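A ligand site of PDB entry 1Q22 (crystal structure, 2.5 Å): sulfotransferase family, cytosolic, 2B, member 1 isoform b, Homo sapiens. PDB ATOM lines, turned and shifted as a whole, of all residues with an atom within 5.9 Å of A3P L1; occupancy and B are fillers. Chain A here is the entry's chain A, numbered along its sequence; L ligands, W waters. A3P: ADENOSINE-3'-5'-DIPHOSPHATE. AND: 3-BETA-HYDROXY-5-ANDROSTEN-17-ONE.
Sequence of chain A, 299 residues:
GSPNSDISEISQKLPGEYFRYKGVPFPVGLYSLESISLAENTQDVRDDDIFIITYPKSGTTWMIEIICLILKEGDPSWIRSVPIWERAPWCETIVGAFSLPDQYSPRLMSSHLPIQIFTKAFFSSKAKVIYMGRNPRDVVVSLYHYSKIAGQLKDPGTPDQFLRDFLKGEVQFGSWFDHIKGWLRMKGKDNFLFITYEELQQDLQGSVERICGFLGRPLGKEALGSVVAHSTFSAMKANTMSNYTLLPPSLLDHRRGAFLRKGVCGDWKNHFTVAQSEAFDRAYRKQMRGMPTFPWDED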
ATOM      1  N   THR A  54     -32.974  -0.186   2.660  1.00  0.00           N
ATOM      2  CA  THR A  54     -33.081  -0.218   1.205  1.00  0.00           C
ATOM      3  C   THR A  54     -34.410  -0.830   0.758  1.00  0.00           C
ATOM      4  O   THR A  54     -35.118  -1.483   1.541  1.00  0.00           O
ATOM      5  CB  THR A  54     -31.976  -1.141   0.582  1.00  0.00           C
ATOM      6  OG1 THR A  54     -32.219  -2.498   0.954  1.00  0.00           O
ATOM      7  CG2 THR A  54     -30.580  -0.745   1.057  1.00  0.00           C
ATOM      8  N   TYR A  55     -34.733  -0.603  -0.505  1.00  0.00           N
ATOM      9  CA  TYR A  55     -35.900  -1.241  -1.114  1.00  0.00           C
ATOM     10  C   TYR A  55     -35.187  -2.493  -1.699  1.00  0.00           C
ATOM     11  O   TYR A  55     -34.095  -2.373  -2.275  1.00  0.00           O
ATOM     12  CB  TYR A  55     -36.471  -0.375  -2.238  1.00  0.00           C
ATOM     13  CG  TYR A  55     -37.681  -0.991  -2.910  1.00  0.00           C
ATOM     14  CD1 TYR A  55     -38.940  -0.923  -2.332  1.00  0.00           C
ATOM     15  CD2 TYR A  55     -37.550  -1.690  -4.125  1.00  0.00           C
ATOM     16  CE1 TYR A  55     -40.050  -1.546  -2.921  1.00  0.00           C
ATOM     17  CE2 TYR A  55     -38.646  -2.316  -4.717  1.00  0.00           C
ATOM     18  CZ  TYR A  55     -39.891  -2.241  -4.111  1.00  0.00           C
ATOM     19  OH  TYR A  55     -40.976  -2.873  -4.674  1.00  0.00           O
ATOM     20  N   PRO A  56     -35.767  -3.690  -1.557  1.00  0.00           N
ATOM     21  CA  PRO A  56     -35.155  -4.922  -2.073  1.00  0.00           C
ATOM     22  C   PRO A  56     -34.449  -4.840  -3.431  1.00  0.00           C
ATOM     23  O   PRO A  56     -34.909  -4.147  -4.354  1.00  0.00           O
ATOM     24  CB  PRO A  56     -36.340  -5.889  -2.103  1.00  0.00           C
ATOM     25  CG  PRO A  56     -37.102  -5.479  -0.870  1.00  0.00           C
ATOM     26  CD  PRO A  56     -37.100  -3.962  -0.980  1.00  0.00           C
ATOM     27  N   LYS A  57     -33.316  -5.528  -3.530  1.00  0.00           N
ATOM     28  CA  LYS A  57     -32.514  -5.599  -4.746  1.00  0.00           C
ATOM     29  C   LYS A  57     -31.776  -4.337  -5.155  1.00  0.00           C
ATOM     30  O   LYS A  57     -31.461  -4.158  -6.342  1.00  0.00           O
ATOM     31  CB  LYS A  57     -33.379  -6.064  -5.928  1.00  0.00           C
ATOM     32  CG  LYS A  57     -34.402  -7.133  -5.576  1.00  0.00           C
ATOM     33  CD  LYS A  57     -33.833  -8.183  -4.627  1.00  0.00           C
ATOM     34  CE  LYS A  57     -32.630  -8.938  -5.214  1.00  0.00           C
ATOM     35  NZ  LYS A  57     -32.035  -9.874  -4.214  1.00  0.00           N
ATOM     36  N   SER A  58     -31.485  -3.464  -4.200  1.00  0.00           N
ATOM     37  CA  SER A  58     -30.779  -2.220  -4.531  1.00  0.00           C
ATOM     38  C   SER A  58     -29.283  -2.330  -4.235  1.00  0.00           C
ATOM     39  O   SER A  58     -28.521  -1.388  -4.482  1.00  0.00           O
ATOM     40  CB  SER A  58     -31.357  -1.037  -3.744  1.00  0.00           C
ATOM     41  OG  SER A  58     -32.708  -0.801  -4.103  1.00  0.00           O
ATOM     42  N   GLY A  59     -28.867  -3.467  -3.701  1.00  0.00           N
ATOM     43  CA  GLY A  59     -27.459  -3.657  -3.386  1.00  0.00           C
ATOM     44  C   GLY A  59     -27.215  -3.627  -1.895  1.00  0.00           C
ATOM     45  O   GLY A  59     -26.188  -3.152  -1.436  1.00  0.00           O
ATOM     46  N   THR A  60     -28.191  -4.138  -1.150  1.00  0.00           N
ATOM     47  CA  THR A  60     -28.100  -4.204   0.303  1.00  0.00           C
ATOM     48  C   THR A  60     -26.839  -5.001   0.643  1.00  0.00           C
ATOM     49  O   THR A  60     -25.966  -4.528   1.375  1.00  0.00           O
ATOM     50  CB  THR A  60     -29.299  -4.966   0.908  1.00  0.00           C
ATOM     51  OG1 THR A  60     -30.518  -4.500   0.320  1.00  0.00           O
ATOM     52  CG2 THR A  60     -29.358  -4.749   2.416  1.00  0.00           C
ATOM     53  N   THR A  61     -26.746  -6.214   0.090  1.00  0.00           N
ATOM     54  CA  THR A  61     -25.599  -7.073   0.332  1.00  0.00           C
ATOM     55  C   THR A  61     -24.305  -6.308   0.168  1.00  0.00           C
ATOM     56  O   THR A  61     -23.435  -6.369   1.016  1.00  0.00           O
ATOM     57  CB  THR A  61     -25.610  -8.300  -0.618  1.00  0.00           C
ATOM     58  OG1 THR A  61     -26.824  -9.046  -0.429  1.00  0.00           O
ATOM     59  CG2 THR A  61     -24.426  -9.225  -0.319  1.00  0.00           C
ATOM     60  N   TRP A  62     -24.168  -5.560  -0.920  1.00  0.00           N
ATOM     61  CA  TRP A  62     -22.962  -4.802  -1.160  1.00  0.00           C
ATOM     62  C   TRP A  62     -22.695  -3.845   0.030  1.00  0.00           C
ATOM     63  O   TRP A  62     -21.590  -3.832   0.587  1.00  0.00           O
ATOM     64  CB  TRP A  62     -23.106  -4.030  -2.461  1.00  0.00           C
ATOM     65  CG  TRP A  62     -21.844  -3.462  -3.038  1.00  0.00           C
ATOM     66  CD1 TRP A  62     -20.602  -3.483  -2.495  1.00  0.00           C
ATOM     67  CD2 TRP A  62     -21.720  -2.782  -4.304  1.00  0.00           C
ATOM     68  NE1 TRP A  62     -19.693  -2.863  -3.345  1.00  0.00           N
ATOM     69  CE2 TRP A  62     -20.356  -2.426  -4.453  1.00  0.00           C
ATOM     70  CE3 TRP A  62     -22.634  -2.440  -5.310  1.00  0.00           C
ATOM     71  CZ2 TRP A  62     -19.883  -1.751  -5.590  1.00  0.00           C
ATOM     72  CZ3 TRP A  62     -22.159  -1.764  -6.437  1.00  0.00           C
ATOM     73  CH2 TRP A  62     -20.792  -1.421  -6.566  1.00  0.00           C
ATOM     74  N   HIS A 112     -35.767  -3.559   5.158  1.00  0.00           N
ATOM     75  CA  HIS A 112     -36.402  -3.188   3.895  1.00  0.00           C
ATOM     76  C   HIS A 112     -37.714  -2.407   4.136  1.00  0.00           C
ATOM     77  O   HIS A 112     -38.428  -2.073   3.195  1.00  0.00           O
ATOM     78  CB  HIS A 112     -36.708  -4.430   3.052  1.00  0.00           C
ATOM     79  CG  HIS A 112     -35.518  -5.025   2.378  1.00  0.00           C
ATOM     80  ND1 HIS A 112     -34.502  -4.254   1.837  1.00  0.00           N
ATOM     81  CD2 HIS A 112     -35.167  -6.314   2.157  1.00  0.00           C
ATOM     82  CE1 HIS A 112     -33.592  -5.043   1.306  1.00  0.00           C
ATOM     83  NE2 HIS A 112     -33.970  -6.294   1.484  1.00  0.00           N
ATOM     84  N   ARG A 134     -31.234   2.435  -5.900  1.00  0.00           N
ATOM     85  CA  ARG A 134     -30.711   1.927  -7.166  1.00  0.00           C
ATOM     86  C   ARG A 134     -31.682   2.312  -8.285  1.00  0.00           C
ATOM     87  O   ARG A 134     -32.823   2.657  -8.016  1.00  0.00           O
ATOM     88  CB  ARG A 134     -30.564   0.400  -7.104  1.00  0.00           C
ATOM     89  CG  ARG A 134     -29.887  -0.247  -8.321  1.00  0.00           C
ATOM     90  CD  ARG A 134     -29.725  -1.761  -8.150  1.00  0.00           C
ATOM     91  NE  ARG A 134     -28.916  -2.338  -9.222  1.00  0.00           N
ATOM     92  CZ  ARG A 134     -28.773  -3.642  -9.454  1.00  0.00           C
ATOM     93  NH1 ARG A 134     -29.396  -4.530  -8.687  1.00  0.00           N
ATOM     94  NH2 ARG A 134     -28.015  -4.064 -10.453  1.00  0.00           N
ATOM     95  N   ASP A 138     -33.242  -1.335 -13.001  1.00  0.00           N
ATOM     96  CA  ASP A 138     -32.324  -2.408 -12.676  1.00  0.00           C
ATOM     97  C   ASP A 138     -32.850  -3.201 -11.492  1.00  0.00           C
ATOM     98  O   ASP A 138     -32.512  -4.374 -11.319  1.00  0.00           O
ATOM     99  CB  ASP A 138     -30.932  -1.864 -12.349  1.00  0.00           C
ATOM    100  CG  ASP A 138     -30.165  -1.460 -13.601  1.00  0.00           C
ATOM    101  OD1 ASP A 138     -30.418  -2.045 -14.667  1.00  0.00           O
ATOM    102  OD2 ASP A 138     -29.298  -0.559 -13.508  1.00  0.00           O
ATOM    103  N   VAL A 141     -35.381  -5.782 -12.817  1.00  0.00           N
ATOM    104  CA  VAL A 141     -34.720  -6.934 -13.408  1.00  0.00           C
ATOM    105  C   VAL A 141     -34.201  -7.859 -12.322  1.00  0.00           C
ATOM    106  O   VAL A 141     -34.570  -9.042 -12.271  1.00  0.00           O
ATOM    107  CB  VAL A 141     -33.512  -6.528 -14.273  1.00  0.00           C
ATOM    108  CG1 VAL A 141     -32.957  -7.760 -14.982  1.00  0.00           C
ATOM    109  CG2 VAL A 141     -33.912  -5.485 -15.284  1.00  0.00           C
ATOM    110  N   SER A 142     -33.352  -7.316 -11.456  1.00  0.00           N
ATOM    111  CA  SER A 142     -32.783  -8.068 -10.357  1.00  0.00           C
ATOM    112  C   SER A 142     -33.855  -8.851  -9.592  1.00  0.00           C
ATOM    113  O   SER A 142     -33.696 -10.051  -9.343  1.00  0.00           O
ATOM    114  CB  SER A 142     -32.058  -7.114  -9.406  1.00  0.00           C
ATOM    115  OG  SER A 142     -31.529  -7.810  -8.292  1.00  0.00           O
ATOM    116  N   LEU A 143     -34.941  -8.173  -9.257  1.00  0.00           N
ATOM    117  CA  LEU A 143     -36.042  -8.775  -8.525  1.00  0.00           C
ATOM    118  C   LEU A 143     -36.798  -9.842  -9.313  1.00  0.00           C
ATOM    119  O   LEU A 143     -37.295 -10.819  -8.738  1.00  0.00           O
ATOM    120  CB  LEU A 143     -37.029  -7.674  -8.085  1.00  0.00           C
ATOM    121  CG  LEU A 143     -38.263  -8.117  -7.295  1.00  0.00           C
ATOM    122  CD1 LEU A 143     -37.826  -8.691  -5.955  1.00  0.00           C
ATOM    123  CD2 LEU A 143     -39.198  -6.932  -7.082  1.00  0.00           C
ATOM    124  N   TYR A 197     -26.542   2.833  -5.522  1.00  0.00           N
ATOM    125  CA  TYR A 197     -25.849   1.705  -6.119  1.00  0.00           C
ATOM    126  C   TYR A 197     -24.969   2.221  -7.285  1.00  0.00           C
ATOM    127  O   TYR A 197     -23.889   1.671  -7.553  1.00  0.00           O
ATOM    128  CB  TYR A 197     -26.889   0.718  -6.654  1.00  0.00           C
ATOM    129  CG  TYR A 197     -26.314  -0.501  -7.348  1.00  0.00           C
ATOM    130  CD1 TYR A 197     -25.991  -1.648  -6.633  1.00  0.00           C
ATOM    131  CD2 TYR A 197     -26.047  -0.479  -8.712  1.00  0.00           C
ATOM    132  CE1 TYR A 197     -25.419  -2.739  -7.250  1.00  0.00           C
ATOM    133  CE2 TYR A 197     -25.465  -1.573  -9.352  1.00  0.00           C
ATOM    134  CZ  TYR A 197     -25.154  -2.694  -8.605  1.00  0.00           C
ATOM    135  OH  TYR A 197     -24.550  -3.774  -9.209  1.00  0.00           O
ATOM    136  N   GLN A 201     -20.752   1.964  -7.898  1.00  0.00           N
ATOM    137  CA  GLN A 201     -20.275   1.358  -9.131  1.00  0.00           C
ATOM    138  C   GLN A 201     -19.292   2.270  -9.855  1.00  0.00           C
ATOM    139  O   GLN A 201     -18.342   1.805 -10.480  1.00  0.00           O
ATOM    140  CB  GLN A 201     -21.455   1.049 -10.057  1.00  0.00           C
ATOM    141  CG  GLN A 201     -22.208  -0.208  -9.696  1.00  0.00           C
ATOM    142  CD  GLN A 201     -21.541  -1.458 -10.253  1.00  0.00           C
ATOM    143  OE1 GLN A 201     -20.377  -1.428 -10.635  1.00  0.00           O
ATOM    144  NE2 GLN A 201     -22.277  -2.554 -10.300  1.00  0.00           N
ATOM    145  N   SER A 231     -14.904  -5.755  -1.156  1.00  0.00           N
ATOM    146  CA  SER A 231     -16.285  -5.365  -1.414  1.00  0.00           C
ATOM    147  C   SER A 231     -16.669  -5.537  -2.872  1.00  0.00           C
ATOM    148  O   SER A 231     -17.843  -5.483  -3.226  1.00  0.00           O
ATOM    149  CB  SER A 231     -16.519  -3.907  -1.009  1.00  0.00           C
ATOM    150  OG  SER A 231     -16.561  -3.793   0.399  1.00  0.00           O
ATOM    151  N   THR A 232     -15.659  -5.753  -3.703  1.00  0.00           N
ATOM    152  CA  THR A 232     -15.865  -5.934  -5.133  1.00  0.00           C
ATOM    153  C   THR A 232     -16.744  -7.135  -5.443  1.00  0.00           C
ATOM    154  O   THR A 232     -16.672  -8.164  -4.769  1.00  0.00           O
ATOM    155  CB  THR A 232     -14.510  -6.032  -5.840  1.00  0.00           C
ATOM    156  OG1 THR A 232     -13.767  -4.841  -5.554  1.00  0.00           O
ATOM    157  CG2 THR A 232     -14.687  -6.149  -7.329  1.00  0.00           C
ATOM    158  N   PHE A 233     -17.576  -6.992  -6.476  1.00  0.00           N
ATOM    159  CA  PHE A 233     -18.490  -8.047  -6.899  1.00  0.00           C
ATOM    160  C   PHE A 233     -17.787  -9.408  -7.040  1.00  0.00           C
ATOM    161  O   PHE A 233     -18.240 -10.414  -6.481  1.00  0.00           O
ATOM    162  CB  PHE A 233     -19.170  -7.666  -8.215  1.00  0.00           C
ATOM    163  CG  PHE A 233     -20.169  -8.691  -8.694  1.00  0.00           C
ATOM    164  CD1 PHE A 233     -21.416  -8.816  -8.089  1.00  0.00           C
ATOM    165  CD2 PHE A 233     -19.829  -9.579  -9.725  1.00  0.00           C
ATOM    166  CE1 PHE A 233     -22.310  -9.821  -8.487  1.00  0.00           C
ATOM    167  CE2 PHE A 233     -20.718 -10.578 -10.135  1.00  0.00           C
ATOM    168  CZ  PHE A 233     -21.967 -10.694  -9.510  1.00  0.00           C
ATOM    169  N   MET A 236     -16.827 -10.732  -3.646  1.00  0.00           N
ATOM    170  CA  MET A 236     -18.017 -11.076  -2.898  1.00  0.00           C
ATOM    171  C   MET A 236     -18.720 -12.344  -3.382  1.00  0.00           C
ATOM    172  O   MET A 236     -19.240 -13.122  -2.577  1.00  0.00           O
ATOM    173  CB  MET A 236     -18.995  -9.893  -2.881  1.00  0.00           C
ATOM    174  CG  MET A 236     -18.605  -8.816  -1.873  1.00  0.00           C
ATOM    175  SD  MET A 236     -19.815  -7.475  -1.626  1.00  0.00           S
ATOM    176  CE  MET A 236     -21.128  -8.377  -0.800  1.00  0.00           C
ATOM    177  N   TYR A 244     -24.604 -16.205  -0.080  1.00  0.00           N
ATOM    178  CA  TYR A 244     -25.794 -16.982   0.228  1.00  0.00           C
ATOM    179  C   TYR A 244     -25.859 -18.440  -0.264  1.00  0.00           C
ATOM    180  O   TYR A 244     -26.918 -19.061  -0.211  1.00  0.00           O
ATOM    181  CB  TYR A 244     -27.016 -16.239  -0.290  1.00  0.00           C
ATOM    182  CG  TYR A 244     -27.235 -14.921   0.394  1.00  0.00           C
ATOM    183  CD1 TYR A 244     -27.795 -14.851   1.666  1.00  0.00           C
ATOM    184  CD2 TYR A 244     -26.897 -13.732  -0.233  1.00  0.00           C
ATOM    185  CE1 TYR A 244     -28.018 -13.630   2.294  1.00  0.00           C
ATOM    186  CE2 TYR A 244     -27.114 -12.505   0.383  1.00  0.00           C
ATOM    187  CZ  TYR A 244     -27.673 -12.458   1.636  1.00  0.00           C
ATOM    188  OH  TYR A 244     -27.927 -11.243   2.219  1.00  0.00           O
ATOM    189  N   PHE A 259     -27.560 -15.491  -5.894  1.00  0.00           N
ATOM    190  CA  PHE A 259     -28.057 -14.241  -5.319  1.00  0.00           C
ATOM    191  C   PHE A 259     -27.312 -13.098  -5.988  1.00  0.00           C
ATOM    192  O   PHE A 259     -27.931 -12.101  -6.366  1.00  0.00           O
ATOM    193  CB  PHE A 259     -27.817 -14.203  -3.817  1.00  0.00           C
ATOM    194  CG  PHE A 259     -28.521 -13.067  -3.126  1.00  0.00           C
ATOM    195  CD1 PHE A 259     -29.697 -13.287  -2.408  1.00  0.00           C
ATOM    196  CD2 PHE A 259     -27.989 -11.777  -3.162  1.00  0.00           C
ATOM    197  CE1 PHE A 259     -30.339 -12.239  -1.735  1.00  0.00           C
ATOM    198  CE2 PHE A 259     -28.616 -10.732  -2.492  1.00  0.00           C
ATOM    199  CZ  PHE A 259     -29.786 -10.960  -1.774  1.00  0.00           C
ATOM    200  N   LEU A 260     -25.994 -13.228  -6.107  1.00  0.00           N
ATOM    201  CA  LEU A 260     -25.221 -12.189  -6.777  1.00  0.00           C
ATOM    202  C   LEU A 260     -25.202 -12.548  -8.261  1.00  0.00           C
ATOM    203  O   LEU A 260     -24.252 -13.161  -8.757  1.00  0.00           O
ATOM    204  CB  LEU A 260     -23.791 -12.122  -6.232  1.00  0.00           C
ATOM    205  CG  LEU A 260     -23.667 -11.782  -4.743  1.00  0.00           C
ATOM    206  CD1 LEU A 260     -22.222 -11.460  -4.417  1.00  0.00           C
ATOM    207  CD2 LEU A 260     -24.529 -10.605  -4.402  1.00  0.00           C
ATOM    208  N   ARG A 261     -26.266 -12.147  -8.946  1.00  0.00           N
ATOM    209  CA  ARG A 261     -26.491 -12.418 -10.368  1.00  0.00           C
ATOM    210  C   ARG A 261     -25.478 -11.831 -11.378  1.00  0.00           C
ATOM    211  O   ARG A 261     -24.694 -12.583 -11.949  1.00  0.00           O
ATOM    212  CB  ARG A 261     -27.913 -11.986 -10.723  1.00  0.00           C
ATOM    213  CG  ARG A 261     -28.423 -12.475 -12.051  1.00  0.00           C
ATOM    214  CD  ARG A 261     -29.845 -12.013 -12.194  1.00  0.00           C
ATOM    215  NE  ARG A 261     -29.916 -10.554 -12.257  1.00  0.00           N
ATOM    216  CZ  ARG A 261     -29.677  -9.866 -13.371  1.00  0.00           C
ATOM    217  NH1 ARG A 261     -29.374 -10.511 -14.488  1.00  0.00           N
ATOM    218  NH2 ARG A 261     -29.719  -8.542 -13.362  1.00  0.00           N
ATOM    219  N   LYS A 262     -25.527 -10.525 -11.632  1.00  0.00           N
ATOM    220  CA  LYS A 262     -24.576  -9.903 -12.571  1.00  0.00           C
ATOM    221  C   LYS A 262     -23.740  -8.787 -11.943  1.00  0.00           C
ATOM    222  O   LYS A 262     -22.538  -8.675 -12.224  1.00  0.00           O
ATOM    223  CB  LYS A 262     -25.294  -9.324 -13.787  1.00  0.00           C
ATOM    224  CG  LYS A 262     -25.513 -10.303 -14.893  1.00  0.00           C
ATOM    225  CD  LYS A 262     -26.066  -9.626 -16.124  1.00  0.00           C
ATOM    226  CE  LYS A 262     -25.064  -8.626 -16.693  1.00  0.00           C
ATOM    227  NZ  LYS A 262     -25.500  -8.175 -18.047  1.00  0.00           N
ATOM    228  N   GLY A 263     -24.390  -7.944 -11.147  1.00  0.00           N
ATOM    229  CA  GLY A 263     -23.664  -6.875 -10.486  1.00  0.00           C
ATOM    230  C   GLY A 263     -23.271  -5.688 -11.336  1.00  0.00           C
ATOM    231  O   GLY A 263     -22.195  -5.139 -11.155  1.00  0.00           O
ATOM    232  N   VAL A 264     -24.131  -5.276 -12.264  1.00  0.00           N
ATOM    233  CA  VAL A 264     -23.803  -4.114 -13.091  1.00  0.00           C
ATOM    234  C   VAL A 264     -24.939  -3.091 -13.128  1.00  0.00           C
ATOM    235  O   VAL A 264     -25.971  -3.263 -12.459  1.00  0.00           O
ATOM    236  CB  VAL A 264     -23.480  -4.542 -14.527  1.00  0.00           C
ATOM    237  CG1 VAL A 264     -22.264  -5.451 -14.539  1.00  0.00           C
ATOM    238  CG2 VAL A 264     -24.661  -5.264 -15.139  1.00  0.00           C
ATOM    239  N   ASP A 267     -28.540  -3.320 -16.793  1.00  0.00           N
ATOM    240  CA  ASP A 267     -28.981  -4.591 -17.315  1.00  0.00           C
ATOM    241  C   ASP A 267     -30.427  -4.478 -17.773  1.00  0.00           C
ATOM    242  O   ASP A 267     -30.912  -5.283 -18.573  1.00  0.00           O
ATOM    243  CB  ASP A 267     -28.888  -5.712 -16.284  1.00  0.00           C
ATOM    244  CG  ASP A 267     -29.016  -7.078 -16.921  1.00  0.00           C
ATOM    245  OD1 ASP A 267     -29.528  -8.011 -16.264  1.00  0.00           O
ATOM    246  OD2 ASP A 267     -28.571  -7.217 -18.087  1.00  0.00           O
HETATM  247  P1  A3P L   1     -28.286  -8.058  -9.885  1.00  0.00           P
HETATM  248  O1P A3P L   1     -29.442  -8.985  -9.708  1.00  0.00           O
HETATM  249  O2P A3P L   1     -27.055  -8.791 -10.214  1.00  0.00           O
HETATM  250  O3P A3P L   1     -28.556  -7.032 -10.889  1.00  0.00           O
HETATM  251  P2  A3P L   1     -29.916  -6.854  -2.567  1.00  0.00           P
HETATM  252  O4P A3P L   1     -30.482  -5.582  -2.112  1.00  0.00           O
HETATM  253  O5P A3P L   1     -28.752  -7.194  -1.741  1.00  0.00           O
HETATM  254  O6P A3P L   1     -30.934  -7.939  -2.532  1.00  0.00           O
HETATM  255  O5' A3P L   1     -29.434  -6.649  -4.062  1.00  0.00           O
HETATM  256  C5' A3P L   1     -28.868  -7.689  -4.874  1.00  0.00           C
HETATM  257  C4' A3P L   1     -28.280  -7.031  -6.124  1.00  0.00           C
HETATM  258  O4' A3P L   1     -27.083  -6.289  -5.719  1.00  0.00           O
HETATM  259  C3' A3P L   1     -27.824  -7.989  -7.214  1.00  0.00           C
HETATM  260  O3' A3P L   1     -28.032  -7.328  -8.489  1.00  0.00           O
HETATM  261  C2' A3P L   1     -26.367  -8.174  -6.837  1.00  0.00           C
HETATM  262  O2' A3P L   1     -25.521  -8.706  -7.816  1.00  0.00           O
HETATM  263  C1' A3P L   1     -25.990  -6.734  -6.494  1.00  0.00           C
HETATM  264  N9  A3P L   1     -24.737  -6.679  -5.753  1.00  0.00           N
HETATM  265  C8  A3P L   1     -24.447  -7.166  -4.492  1.00  0.00           C
HETATM  266  N7  A3P L   1     -23.208  -6.976  -4.111  1.00  0.00           N
HETATM  267  C5  A3P L   1     -22.634  -6.332  -5.184  1.00  0.00           C
HETATM  268  C6  A3P L   1     -21.321  -5.832  -5.421  1.00  0.00           C
HETATM  269  N6  A3P L   1     -20.338  -5.950  -4.541  1.00  0.00           N
HETATM  270  N1  A3P L   1     -21.079  -5.221  -6.615  1.00  0.00           N
HETATM  271  C2  A3P L   1     -22.066  -5.091  -7.526  1.00  0.00           C
HETATM  272  N3  A3P L   1     -23.341  -5.527  -7.420  1.00  0.00           N
HETATM  273  C4  A3P L   1     -23.564  -6.125  -6.211  1.00  0.00           C
HETATM  274  C1  AND L   2     -34.620 -11.103   3.830  1.00  0.00           C
HETATM  275  C2  AND L   2     -34.574  -9.976   2.762  1.00  0.00           C
HETATM  276  C3  AND L   2     -33.131  -9.688   2.215  1.00  0.00           C
HETATM  277  O3  AND L   2     -33.133  -8.601   1.198  1.00  0.00           O
HETATM  278  C4  AND L   2     -32.467 -10.963   1.619  1.00  0.00           C
HETATM  279  C5  AND L   2     -32.456 -12.107   2.657  1.00  0.00           C
HETATM  280  C6  AND L   2     -31.221 -12.996   2.853  1.00  0.00           C
HETATM  281  C7  AND L   2     -31.160 -14.187   3.843  1.00  0.00           C
HETATM  282  C8  AND L   2     -32.433 -14.500   4.665  1.00  0.00           C
HETATM  283  C9  AND L   2     -33.312 -13.178   4.912  1.00  0.00           C
HETATM  284  C10 AND L   2     -33.760 -12.434   3.526  1.00  0.00           C
HETATM  285  C11 AND L   2     -34.576 -13.539   5.786  1.00  0.00           C
HETATM  286  C12 AND L   2     -34.175 -14.264   7.139  1.00  0.00           C
HETATM  287  C13 AND L   2     -33.327 -15.550   6.937  1.00  0.00           C
HETATM  288  C14 AND L   2     -32.101 -15.165   6.029  1.00  0.00           C
HETATM  289  C15 AND L   2     -31.293 -16.455   6.089  1.00  0.00           C
HETATM  290  C16 AND L   2     -31.289 -16.718   7.628  1.00  0.00           C
HETATM  291  C17 AND L   2     -32.547 -16.169   8.123  1.00  0.00           C
HETATM  292  O17 AND L   2     -32.878 -16.237   9.328  1.00  0.00           O
HETATM  293  C18 AND L   2     -34.302 -16.730   6.440  1.00  0.00           C
HETATM  294  C19 AND L   2     -34.709 -13.409   2.638  1.00  0.00           C
HETATM  295  O   HOH W   1     -31.154 -10.788  -8.756  1.00  0.00           O
HETATM  296  O   HOH W   2     -26.588  -6.435 -12.780  1.00  0.00           O
HETATM  297  O   HOH W   3     -30.497  -8.127   0.297  1.00  0.00           O
HETATM  298  O   HOH W   4     -30.273  -5.487 -12.461  1.00  0.00           O
HETATM  299  O   HOH W   5     -18.477  -4.234  -7.410  1.00  0.00           O
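Water W1 lies within hydrogen-bond range of an oxygen (O1P) of A3P L1 and the backbone carbonyl oxygen (O) of Ser 142.
Water W2 lies within hydrogen-bond range of N of Val 264, O3P of A3P L1 and N of Gly 263.
Water W4 lies within hydrogen-bond range of the backbone carbonyl oxygen of Asp 138 (2.7 Å), an oxygen (O3P) of A3P L1 (2.8 Å), the guanidinium group of Arg 261 (3.2 Å) and the guanidinium group of Arg 134 (3.3 Å).
Water W3 lies within hydrogen-bond range of O3 of AND L2 and O5P of A3P L1.
Water W5 lies within hydrogen-bond range of a nitrogen (N1) of A3P L1 and the backbone NH of Phe 233.
The indole nitrogen (NE1) of Trp 62 lies close to a nitrogen (N6) of A3P L1, at 3.4 Å.
Residues that only touch A3P L1: Gln 201, Thr 232, Phe 233, Phe 259 and Leu 260.
Hydrophobic or aromatic side chains within 4 Å of A3P L1: Trp 62, Tyr 197, Phe 233, Met 236, Phe 259 and Leu 260.
Within 4 Å of A3P L1: Lys 57, Ser 58, Gly 59, Thr 60, Thr 61, Trp 62, Arg 134, Ser 142, Tyr 197, Gln 201, Ser 231, Thr 232, Phe 233, Met 236, Phe 259, Leu 260, Arg 261, Lys 262 and Gly 263.
The nearest printed residue that does not touch A3P L1 is Pro 56 (4.2 Å).
NE2 of His 112 lies within hydrogen-bond range of O3 of AND L2, 2.5 Å away.
The backbone NH (N) of Gly 263 lies within hydrogen-bond range of an oxygen (O2P) of A3P L1.
O of Ser 231 is in hydrogen-bond range of N6 of A3P L1.
N of Lys 262 sits at hydrogen-bond distance from O2P of A3P L1.
An oxygen (O4P) of A3P L1 sits at hydrogen-bond distance from the side-chain hydroxyl (OG1) of Thr 60 (2.7 Å).
O5P of A3P L1 sits at hydrogen-bond distance from N of Thr 61, 2.9 Å away.
The backbone NH of Thr 60 is in hydrogen-bond range of an oxygen (O4P) of A3P L1 (2.9 Å).
The guanidinium group (NE) of Arg 261 lies within salt-bridge range of an oxygen (O1P) of A3P L1 (3.0 Å).
An oxygen (O4P) of A3P L1 lies within hydrogen-bond range of the backbone NH of Ser 58, 3.1 Å away.
The side-chain hydroxyl of Thr 61 is in hydrogen-bond range of an oxygen (O5P) of A3P L1.
The side-chain sulfur (SD) of Met 236 sits at hydrogen-bond distance from a nitrogen (N6) of A3P L1, 3.3 Å away.
O4P of A3P L1 lies within hydrogen-bond range of N of Lys 57, 3.2 Å away.
The side-chain amino group (NZ) of Lys 57 lies within salt-bridge range of an oxygen (O6P) of A3P L1 (2.8 Å).
NH2 of Arg 134 lies within salt-bridge range of O3P of A3P L1 (3.0 Å).
The side-chain hydroxyl (OG) of Ser 142 sits at hydrogen-bond distance from an oxygen (O1P) of A3P L1 (2.8 Å).
The side-chain hydroxyl of Tyr 197 sits at hydrogen-bond distance from a nitrogen (N3) of A3P L1, at 2.8 Å.
The backbone NH (N) of Gly 59 lies within hydrogen-bond range of an oxygen (O4P) of A3P L1 (3.1 Å).
The guanidinium group (NH2) of Arg 134 sits at hydrogen-bond distance from the backbone carbonyl oxygen (O) of Val 264 (3.0 Å).
The side-chain carboxylate of Asp 267 lies within salt-bridge range of the guanidinium group of Arg 261 (3.0 Å).
The backbone carbonyl oxygen (O) of Lys 57 sits at hydrogen-bond distance from the guanidinium group (NH1) of Arg 134 (3.1 Å).
The side-chain hydroxyl of Tyr 197 sits close to the backbone carbonyl oxygen of Gly 263 (3.3 Å).
The side-chain hydroxyl (OH) of Tyr 197 sits at hydrogen-bond distance from the side-chain amide nitrogen (NE2) of Gln 201, at 2.8 Å.
OG of Ser 58 is in hydrogen-bond range of O of Tyr 55, at 2.8 Å.
N of Val 264 lies within hydrogen-bond range of OH of Tyr 197 (3.4 Å).
OD2 of Asp 267 lies within salt-bridge range of NZ of Lys 262, at 3.2 Å.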
